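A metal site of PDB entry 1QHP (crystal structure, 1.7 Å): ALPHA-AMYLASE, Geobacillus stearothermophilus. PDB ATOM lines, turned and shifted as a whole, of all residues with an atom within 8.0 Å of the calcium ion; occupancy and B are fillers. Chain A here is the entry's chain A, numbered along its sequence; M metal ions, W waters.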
ATOM      1  N   PRO A  29      29.495 -23.737  20.837  1.00  0.00           N
ATOM      2  CA  PRO A  29      28.358 -23.479  21.721  1.00  0.00           C
ATOM      3  C   PRO A  29      27.362 -24.617  21.740  1.00  0.00           C
ATOM      4  O   PRO A  29      27.098 -25.235  20.707  1.00  0.00           O
ATOM      5  CB  PRO A  29      27.680 -22.183  21.238  1.00  0.00           C
ATOM      6  CG  PRO A  29      28.659 -21.647  20.247  1.00  0.00           C
ATOM      7  CD  PRO A  29      29.531 -22.779  19.725  1.00  0.00           C
ATOM      8  N   LYS A  31      24.194 -24.345  21.662  1.00  0.00           N
ATOM      9  CA  LYS A  31      23.138 -24.022  20.709  1.00  0.00           C
ATOM     10  C   LYS A  31      23.391 -24.637  19.340  1.00  0.00           C
ATOM     11  O   LYS A  31      22.427 -24.933  18.619  1.00  0.00           O
ATOM     12  CB  LYS A  31      23.018 -22.492  20.586  1.00  0.00           C
ATOM     13  CG  LYS A  31      22.005 -21.983  19.565  1.00  0.00           C
ATOM     14  CD  LYS A  31      21.772 -20.488  19.780  1.00  0.00           C
ATOM     15  CE  LYS A  31      20.835 -19.872  18.753  1.00  0.00           C
ATOM     16  NZ  LYS A  31      21.407 -19.944  17.362  1.00  0.00           N
ATOM     17  N   SER A  32      24.644 -24.754  18.912  1.00  0.00           N
ATOM     18  CA  SER A  32      24.988 -25.302  17.598  1.00  0.00           C
ATOM     19  C   SER A  32      26.224 -26.204  17.721  1.00  0.00           C
ATOM     20  O   SER A  32      27.230 -26.109  17.019  1.00  0.00           O
ATOM     21  CB  SER A  32      25.337 -24.129  16.658  1.00  0.00           C
ATOM     22  OG  SER A  32      26.270 -23.258  17.306  1.00  0.00           O
ATOM     23  N   LEU A  35      29.783 -28.231  15.222  1.00  0.00           N
ATOM     24  CA  LEU A  35      30.100 -27.618  13.934  1.00  0.00           C
ATOM     25  C   LEU A  35      31.494 -27.021  13.911  1.00  0.00           C
ATOM     26  O   LEU A  35      31.901 -26.399  12.919  1.00  0.00           O
ATOM     27  CB  LEU A  35      29.071 -26.497  13.632  1.00  0.00           C
ATOM     28  CG  LEU A  35      27.593 -26.872  13.790  1.00  0.00           C
ATOM     29  CD1 LEU A  35      26.723 -25.695  13.374  1.00  0.00           C
ATOM     30  CD2 LEU A  35      27.247 -28.122  12.987  1.00  0.00           C
ATOM     31  N   TYR A  46      33.255 -24.573  11.151  1.00  0.00           N
ATOM     32  CA  TYR A  46      33.738 -23.358  11.831  1.00  0.00           C
ATOM     33  C   TYR A  46      35.137 -23.629  12.404  1.00  0.00           C
ATOM     34  O   TYR A  46      35.327 -24.670  13.019  1.00  0.00           O
ATOM     35  CB  TYR A  46      32.854 -22.929  12.991  1.00  0.00           C
ATOM     36  CG  TYR A  46      31.518 -22.307  12.677  1.00  0.00           C
ATOM     37  CD1 TYR A  46      30.413 -23.115  12.457  1.00  0.00           C
ATOM     38  CD2 TYR A  46      31.353 -20.925  12.675  1.00  0.00           C
ATOM     39  CE1 TYR A  46      29.173 -22.560  12.194  1.00  0.00           C
ATOM     40  CE2 TYR A  46      30.108 -20.352  12.424  1.00  0.00           C
ATOM     41  CZ  TYR A  46      29.032 -21.187  12.191  1.00  0.00           C
ATOM     42  OH  TYR A  46      27.798 -20.657  11.943  1.00  0.00           O
ATOM     43  N   LEU A  75      24.935 -12.407  11.202  1.00  0.00           N
ATOM     44  CA  LEU A  75      23.688 -12.875  11.824  1.00  0.00           C
ATOM     45  C   LEU A  75      23.601 -14.381  11.948  1.00  0.00           C
ATOM     46  O   LEU A  75      24.359 -15.136  11.351  1.00  0.00           O
ATOM     47  CB  LEU A  75      22.490 -12.251  11.076  1.00  0.00           C
ATOM     48  CG  LEU A  75      22.523 -10.718  11.045  1.00  0.00           C
ATOM     49  CD1 LEU A  75      21.503 -10.136  10.072  1.00  0.00           C
ATOM     50  CD2 LEU A  75      22.291 -10.163  12.466  1.00  0.00           C
ATOM     51  N   ASP A  76      22.762 -14.815  12.889  1.00  0.00           N
ATOM     52  CA  ASP A  76      22.696 -16.221  13.294  1.00  0.00           C
ATOM     53  C   ASP A  76      22.499 -17.156  12.102  1.00  0.00           C
ATOM     54  O   ASP A  76      21.471 -17.080  11.423  1.00  0.00           O
ATOM     55  CB  ASP A  76      21.522 -16.330  14.280  1.00  0.00           C
ATOM     56  CG  ASP A  76      21.325 -17.702  14.881  1.00  0.00           C
ATOM     57  OD1 ASP A  76      22.274 -18.513  14.742  1.00  0.00           O
ATOM     58  OD2 ASP A  76      20.315 -18.022  15.510  1.00  0.00           O
ATOM     59  N   ASN A  77      23.468 -18.041  11.857  1.00  0.00           N
ATOM     60  CA  ASN A  77      23.367 -18.990  10.751  1.00  0.00           C
ATOM     61  C   ASN A  77      22.919 -20.365  11.227  1.00  0.00           C
ATOM     62  O   ASN A  77      22.923 -20.666  12.406  1.00  0.00           O
ATOM     63  CB  ASN A  77      24.741 -19.162  10.078  1.00  0.00           C
ATOM     64  CG  ASN A  77      24.929 -18.229   8.904  1.00  0.00           C
ATOM     65  OD1 ASN A  77      25.445 -18.693   7.872  1.00  0.00           O
ATOM     66  ND2 ASN A  77      24.478 -16.979   9.000  1.00  0.00           N
ATOM     67  N   LEU A  78      22.420 -21.199  10.330  1.00  0.00           N
ATOM     68  CA  LEU A  78      22.111 -22.599  10.541  1.00  0.00           C
ATOM     69  C   LEU A  78      22.831 -23.235  11.726  1.00  0.00           C
ATOM     70  O   LEU A  78      24.065 -23.239  11.779  1.00  0.00           O
ATOM     71  CB  LEU A  78      22.512 -23.335   9.239  1.00  0.00           C
ATOM     72  CG  LEU A  78      22.198 -24.849   9.224  1.00  0.00           C
ATOM     73  CD1 LEU A  78      20.696 -25.072   9.194  1.00  0.00           C
ATOM     74  CD2 LEU A  78      22.897 -25.462   8.005  1.00  0.00           C
ATOM     75  N   ASP A  79      22.061 -23.828  12.650  1.00  0.00           N
ATOM     76  CA  ASP A  79      22.654 -24.443  13.829  1.00  0.00           C
ATOM     77  C   ASP A  79      22.989 -25.918  13.688  1.00  0.00           C
ATOM     78  O   ASP A  79      23.419 -26.542  14.671  1.00  0.00           O
ATOM     79  CB  ASP A  79      21.676 -24.295  15.032  1.00  0.00           C
ATOM     80  CG  ASP A  79      21.665 -22.892  15.579  1.00  0.00           C
ATOM     81  OD1 ASP A  79      22.617 -22.166  15.242  1.00  0.00           O
ATOM     82  OD2 ASP A  79      20.821 -22.418  16.350  1.00  0.00           O
ATOM     83  N   THR A  80      22.769 -26.499  12.526  1.00  0.00           N
ATOM     84  CA  THR A  80      23.044 -27.913  12.260  1.00  0.00           C
ATOM     85  C   THR A  80      24.021 -28.044  11.091  1.00  0.00           C
ATOM     86  O   THR A  80      24.368 -27.058  10.454  1.00  0.00           O
ATOM     87  CB  THR A  80      21.772 -28.674  11.806  1.00  0.00           C
ATOM     88  OG1 THR A  80      21.355 -28.216  10.496  1.00  0.00           O
ATOM     89  CG2 THR A  80      20.593 -28.473  12.747  1.00  0.00           C
ATOM     90  N   GLY A  88      27.413 -23.352   8.216  1.00  0.00           N
ATOM     91  CA  GLY A  88      27.286 -21.939   7.880  1.00  0.00           C
ATOM     92  C   GLY A  88      28.429 -21.098   8.401  1.00  0.00           C
ATOM     93  O   GLY A  88      28.206 -19.899   8.665  1.00  0.00           O
ATOM     94  N   TRP A  93      24.013 -18.392   5.364  1.00  0.00           N
ATOM     95  CA  TRP A  93      22.838 -19.236   5.615  1.00  0.00           C
ATOM     96  C   TRP A  93      22.148 -18.809   6.903  1.00  0.00           C
ATOM     97  O   TRP A  93      22.322 -19.448   7.956  1.00  0.00           O
ATOM     98  CB  TRP A  93      23.266 -20.708   5.695  1.00  0.00           C
ATOM     99  CG  TRP A  93      23.954 -21.268   4.483  1.00  0.00           C
ATOM    100  CD1 TRP A  93      23.936 -20.813   3.196  1.00  0.00           C
ATOM    101  CD2 TRP A  93      24.709 -22.501   4.457  1.00  0.00           C
ATOM    102  NE1 TRP A  93      24.671 -21.659   2.379  1.00  0.00           N
ATOM    103  CE2 TRP A  93      25.146 -22.690   3.143  1.00  0.00           C
ATOM    104  CE3 TRP A  93      25.080 -23.423   5.451  1.00  0.00           C
ATOM    105  CZ2 TRP A  93      25.945 -23.768   2.757  1.00  0.00           C
ATOM    106  CZ3 TRP A  93      25.850 -24.505   5.048  1.00  0.00           C
ATOM    107  CH2 TRP A  93      26.282 -24.673   3.732  1.00  0.00           C
ATOM    108  N   ARG A  95      19.460 -18.129   9.789  1.00  0.00           N
ATOM    109  CA  ARG A  95      18.220 -18.597  10.382  1.00  0.00           C
ATOM    110  C   ARG A  95      17.509 -17.515  11.180  1.00  0.00           C
ATOM    111  O   ARG A  95      16.345 -17.707  11.531  1.00  0.00           O
ATOM    112  CB  ARG A  95      18.471 -19.784  11.319  1.00  0.00           C
ATOM    113  CG  ARG A  95      19.277 -19.463  12.568  1.00  0.00           C
ATOM    114  CD  ARG A  95      19.783 -20.727  13.236  1.00  0.00           C
ATOM    115  NE  ARG A  95      18.792 -21.662  13.746  1.00  0.00           N
ATOM    116  CZ  ARG A  95      18.134 -21.508  14.900  1.00  0.00           C
ATOM    117  NH1 ARG A  95      18.296 -20.431  15.653  1.00  0.00           N
ATOM    118  NH2 ARG A  95      17.318 -22.470  15.319  1.00  0.00           N
ATOM    119  N   ASP A  96      18.234 -16.468  11.612  1.00  0.00           N
ATOM    120  CA  ASP A  96      17.620 -15.435  12.444  1.00  0.00           C
ATOM    121  C   ASP A  96      18.323 -14.120  12.155  1.00  0.00           C
ATOM    122  O   ASP A  96      19.462 -13.919  12.594  1.00  0.00           O
ATOM    123  CB  ASP A  96      17.714 -15.806  13.928  1.00  0.00           C
ATOM    124  CG  ASP A  96      16.885 -14.898  14.832  1.00  0.00           C
ATOM    125  OD1 ASP A  96      16.579 -13.739  14.478  1.00  0.00           O
ATOM    126  OD2 ASP A  96      16.549 -15.359  15.954  1.00  0.00           O
ATOM    127  N   GLN A  99      19.574 -11.717  15.422  1.00  0.00           N
ATOM    128  CA  GLN A  99      20.577 -12.118  16.382  1.00  0.00           C
ATOM    129  C   GLN A  99      21.949 -12.355  15.766  1.00  0.00           C
ATOM    130  O   GLN A  99      22.047 -12.768  14.612  1.00  0.00           O
ATOM    131  CB  GLN A  99      20.226 -13.440  17.101  1.00  0.00           C
ATOM    132  CG  GLN A  99      18.991 -13.329  17.981  1.00  0.00           C
ATOM    133  CD  GLN A  99      19.227 -13.923  19.354  1.00  0.00           C
ATOM    134  OE1 GLN A  99      20.110 -13.451  20.096  1.00  0.00           O
ATOM    135  NE2 GLN A  99      18.448 -14.948  19.678  1.00  0.00           N
ATOM    136  N   ILE A 100      22.975 -12.031  16.562  1.00  0.00           N
ATOM    137  CA  ILE A 100      24.337 -12.275  16.104  1.00  0.00           C
ATOM    138  C   ILE A 100      24.615 -13.765  16.169  1.00  0.00           C
ATOM    139  O   ILE A 100      24.152 -14.469  17.072  1.00  0.00           O
ATOM    140  CB  ILE A 100      25.327 -11.510  17.004  1.00  0.00           C
ATOM    141  CG1 ILE A 100      25.078  -9.998  16.938  1.00  0.00           C
ATOM    142  CG2 ILE A 100      26.778 -11.851  16.699  1.00  0.00           C
ATOM    143  CD1 ILE A 100      25.287  -9.381  15.561  1.00  0.00           C
ATOM    144  N   GLU A 101      25.384 -14.258  15.194  1.00  0.00           N
ATOM    145  CA  GLU A 101      25.791 -15.658  15.219  1.00  0.00           C
ATOM    146  C   GLU A 101      26.572 -15.954  16.492  1.00  0.00           C
ATOM    147  O   GLU A 101      27.571 -15.306  16.793  1.00  0.00           O
ATOM    148  CB  GLU A 101      26.625 -15.933  13.951  1.00  0.00           C
ATOM    149  CG  GLU A 101      27.492 -17.197  14.031  1.00  0.00           C
ATOM    150  CD  GLU A 101      26.650 -18.413  14.326  1.00  0.00           C
ATOM    151  OE1 GLU A 101      25.545 -18.462  13.723  1.00  0.00           O
ATOM    152  OE2 GLU A 101      27.021 -19.288  15.120  1.00  0.00           O
ATOM    153  N   GLU A 102      26.152 -16.981  17.241  1.00  0.00           N
ATOM    154  CA  GLU A 102      26.737 -17.290  18.543  1.00  0.00           C
ATOM    155  C   GLU A 102      28.187 -17.716  18.486  1.00  0.00           C
ATOM    156  O   GLU A 102      28.943 -17.449  19.435  1.00  0.00           O
ATOM    157  CB  GLU A 102      25.901 -18.337  19.312  1.00  0.00           C
ATOM    158  CG  GLU A 102      25.941 -19.751  18.748  1.00  0.00           C
ATOM    159  CD  GLU A 102      25.076 -19.949  17.543  1.00  0.00           C
ATOM    160  OE1 GLU A 102      24.256 -19.068  17.148  1.00  0.00           O
ATOM    161  OE2 GLU A 102      25.158 -21.042  16.923  1.00  0.00           O
ATOM    162  N   HIS A 103      28.687 -18.287  17.382  1.00  0.00           N
ATOM    163  CA  HIS A 103      30.099 -18.582  17.241  1.00  0.00           C
ATOM    164  C   HIS A 103      30.918 -17.286  17.178  1.00  0.00           C
ATOM    165  O   HIS A 103      32.111 -17.319  17.492  1.00  0.00           O
ATOM    166  CB  HIS A 103      30.373 -19.347  15.936  1.00  0.00           C
ATOM    167  CG  HIS A 103      30.021 -20.811  16.020  1.00  0.00           C
ATOM    168  ND1 HIS A 103      28.757 -21.292  15.734  1.00  0.00           N
ATOM    169  CD2 HIS A 103      30.779 -21.883  16.336  1.00  0.00           C
ATOM    170  CE1 HIS A 103      28.762 -22.613  15.893  1.00  0.00           C
ATOM    171  NE2 HIS A 103      29.982 -22.988  16.245  1.00  0.00           N
ATOM    172  N   PHE A 104      30.296 -16.178  16.758  1.00  0.00           N
ATOM    173  CA  PHE A 104      31.019 -14.930  16.599  1.00  0.00           C
ATOM    174  C   PHE A 104      30.893 -13.944  17.753  1.00  0.00           C
ATOM    175  O   PHE A 104      31.770 -13.072  17.852  1.00  0.00           O
ATOM    176  CB  PHE A 104      30.585 -14.247  15.302  1.00  0.00           C
ATOM    177  CG  PHE A 104      30.748 -15.038  14.031  1.00  0.00           C
ATOM    178  CD1 PHE A 104      31.568 -16.144  13.938  1.00  0.00           C
ATOM    179  CD2 PHE A 104      30.103 -14.607  12.876  1.00  0.00           C
ATOM    180  CE1 PHE A 104      31.712 -16.858  12.759  1.00  0.00           C
ATOM    181  CE2 PHE A 104      30.241 -15.296  11.682  1.00  0.00           C
ATOM    182  CZ  PHE A 104      31.043 -16.423  11.619  1.00  0.00           C
ATOM    183  N   GLU A 145      17.733 -27.572   8.771  1.00  0.00           N
ATOM    184  CA  GLU A 145      16.577 -27.074   9.540  1.00  0.00           C
ATOM    185  C   GLU A 145      15.370 -26.827   8.652  1.00  0.00           C
ATOM    186  O   GLU A 145      14.451 -26.064   8.983  1.00  0.00           O
ATOM    187  CB  GLU A 145      16.976 -25.786  10.295  1.00  0.00           C
ATOM    188  CG  GLU A 145      18.005 -26.020  11.379  1.00  0.00           C
ATOM    189  CD  GLU A 145      18.563 -24.769  12.034  1.00  0.00           C
ATOM    190  OE1 GLU A 145      18.075 -23.657  11.794  1.00  0.00           O
ATOM    191  OE2 GLU A 145      19.543 -24.874  12.792  1.00  0.00           O
HETATM  192 CA    CA M   1      24.056 -20.225  14.694  1.00  0.00          CA
HETATM  193  O   HOH W   1      25.722 -21.812  13.544  1.00  0.00           O
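The backbone NH (N) of Asp 76 lies within hydrogen-bond range of the backbone carbonyl oxygen (O) of Gln 99 (2.8 Å). The side-chain amino group (NZ) of Lys 31 lies close to the side-chain carboxylate (OE1) of Glu 102 (3.0 Å). The side-chain amide nitrogen (ND2) of Asn 77 lies within hydrogen-bond range of the backbone carbonyl oxygen (O) of Leu 75. The side-chain carboxylate (OD2) of Asp 79 lies within salt-bridge range of the side-chain amino group (NZ) of Lys 31, 2.7 Å away. OD2 of Asp 76 is in salt-bridge range of NH1 of Arg 95 (3.1 Å). O of Asp 76 lies within hydrogen-bond range of N of Asp 96 (3.3 Å). The side-chain amide oxygen (OD1) of Asn 77 sits at hydrogen-bond distance from the backbone NH (N) of Trp 93, 2.9 Å away. The backbone NH (N) of Asp 79 sits at hydrogen-bond distance from the side-chain carboxylate (OE2) of Glu 145.
Merely in contact with the calcium ion: Lys 31 (3.8 Å). Of the 22 residues printed, 6 come within 4 Å of the calcium ion.
The calcium ion is bound by the side-chain carboxylate (OD1) of Asp 76 (2.5 Å), the side-chain carboxylate (OD1) of Asp 79 (2.5 Å), the side-chain carboxylate (OE1) of Glu 101 (2.5 Å), water W1 (2.6 Å), the backbone carbonyl oxygen (O) of Asn 77 (2.6 Å), the side-chain carboxylate (OE2) of Glu 102 (2.6 Å) and the side-chain carboxylate (OE1) of Glu 102 (2.7 Å). Slightly farther from the calcium ion lies the side-chain carboxylate (OE2) of Glu 101 (3.1 Å).
Water W1 lies within hydrogen-bond range of the backbone carbonyl oxygen of Leu 78 (2.8 Å), the side-chain hydroxyl of Tyr 46 (2.9 Å) and the side-chain carboxylate of Glu 101 (3.2 Å).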
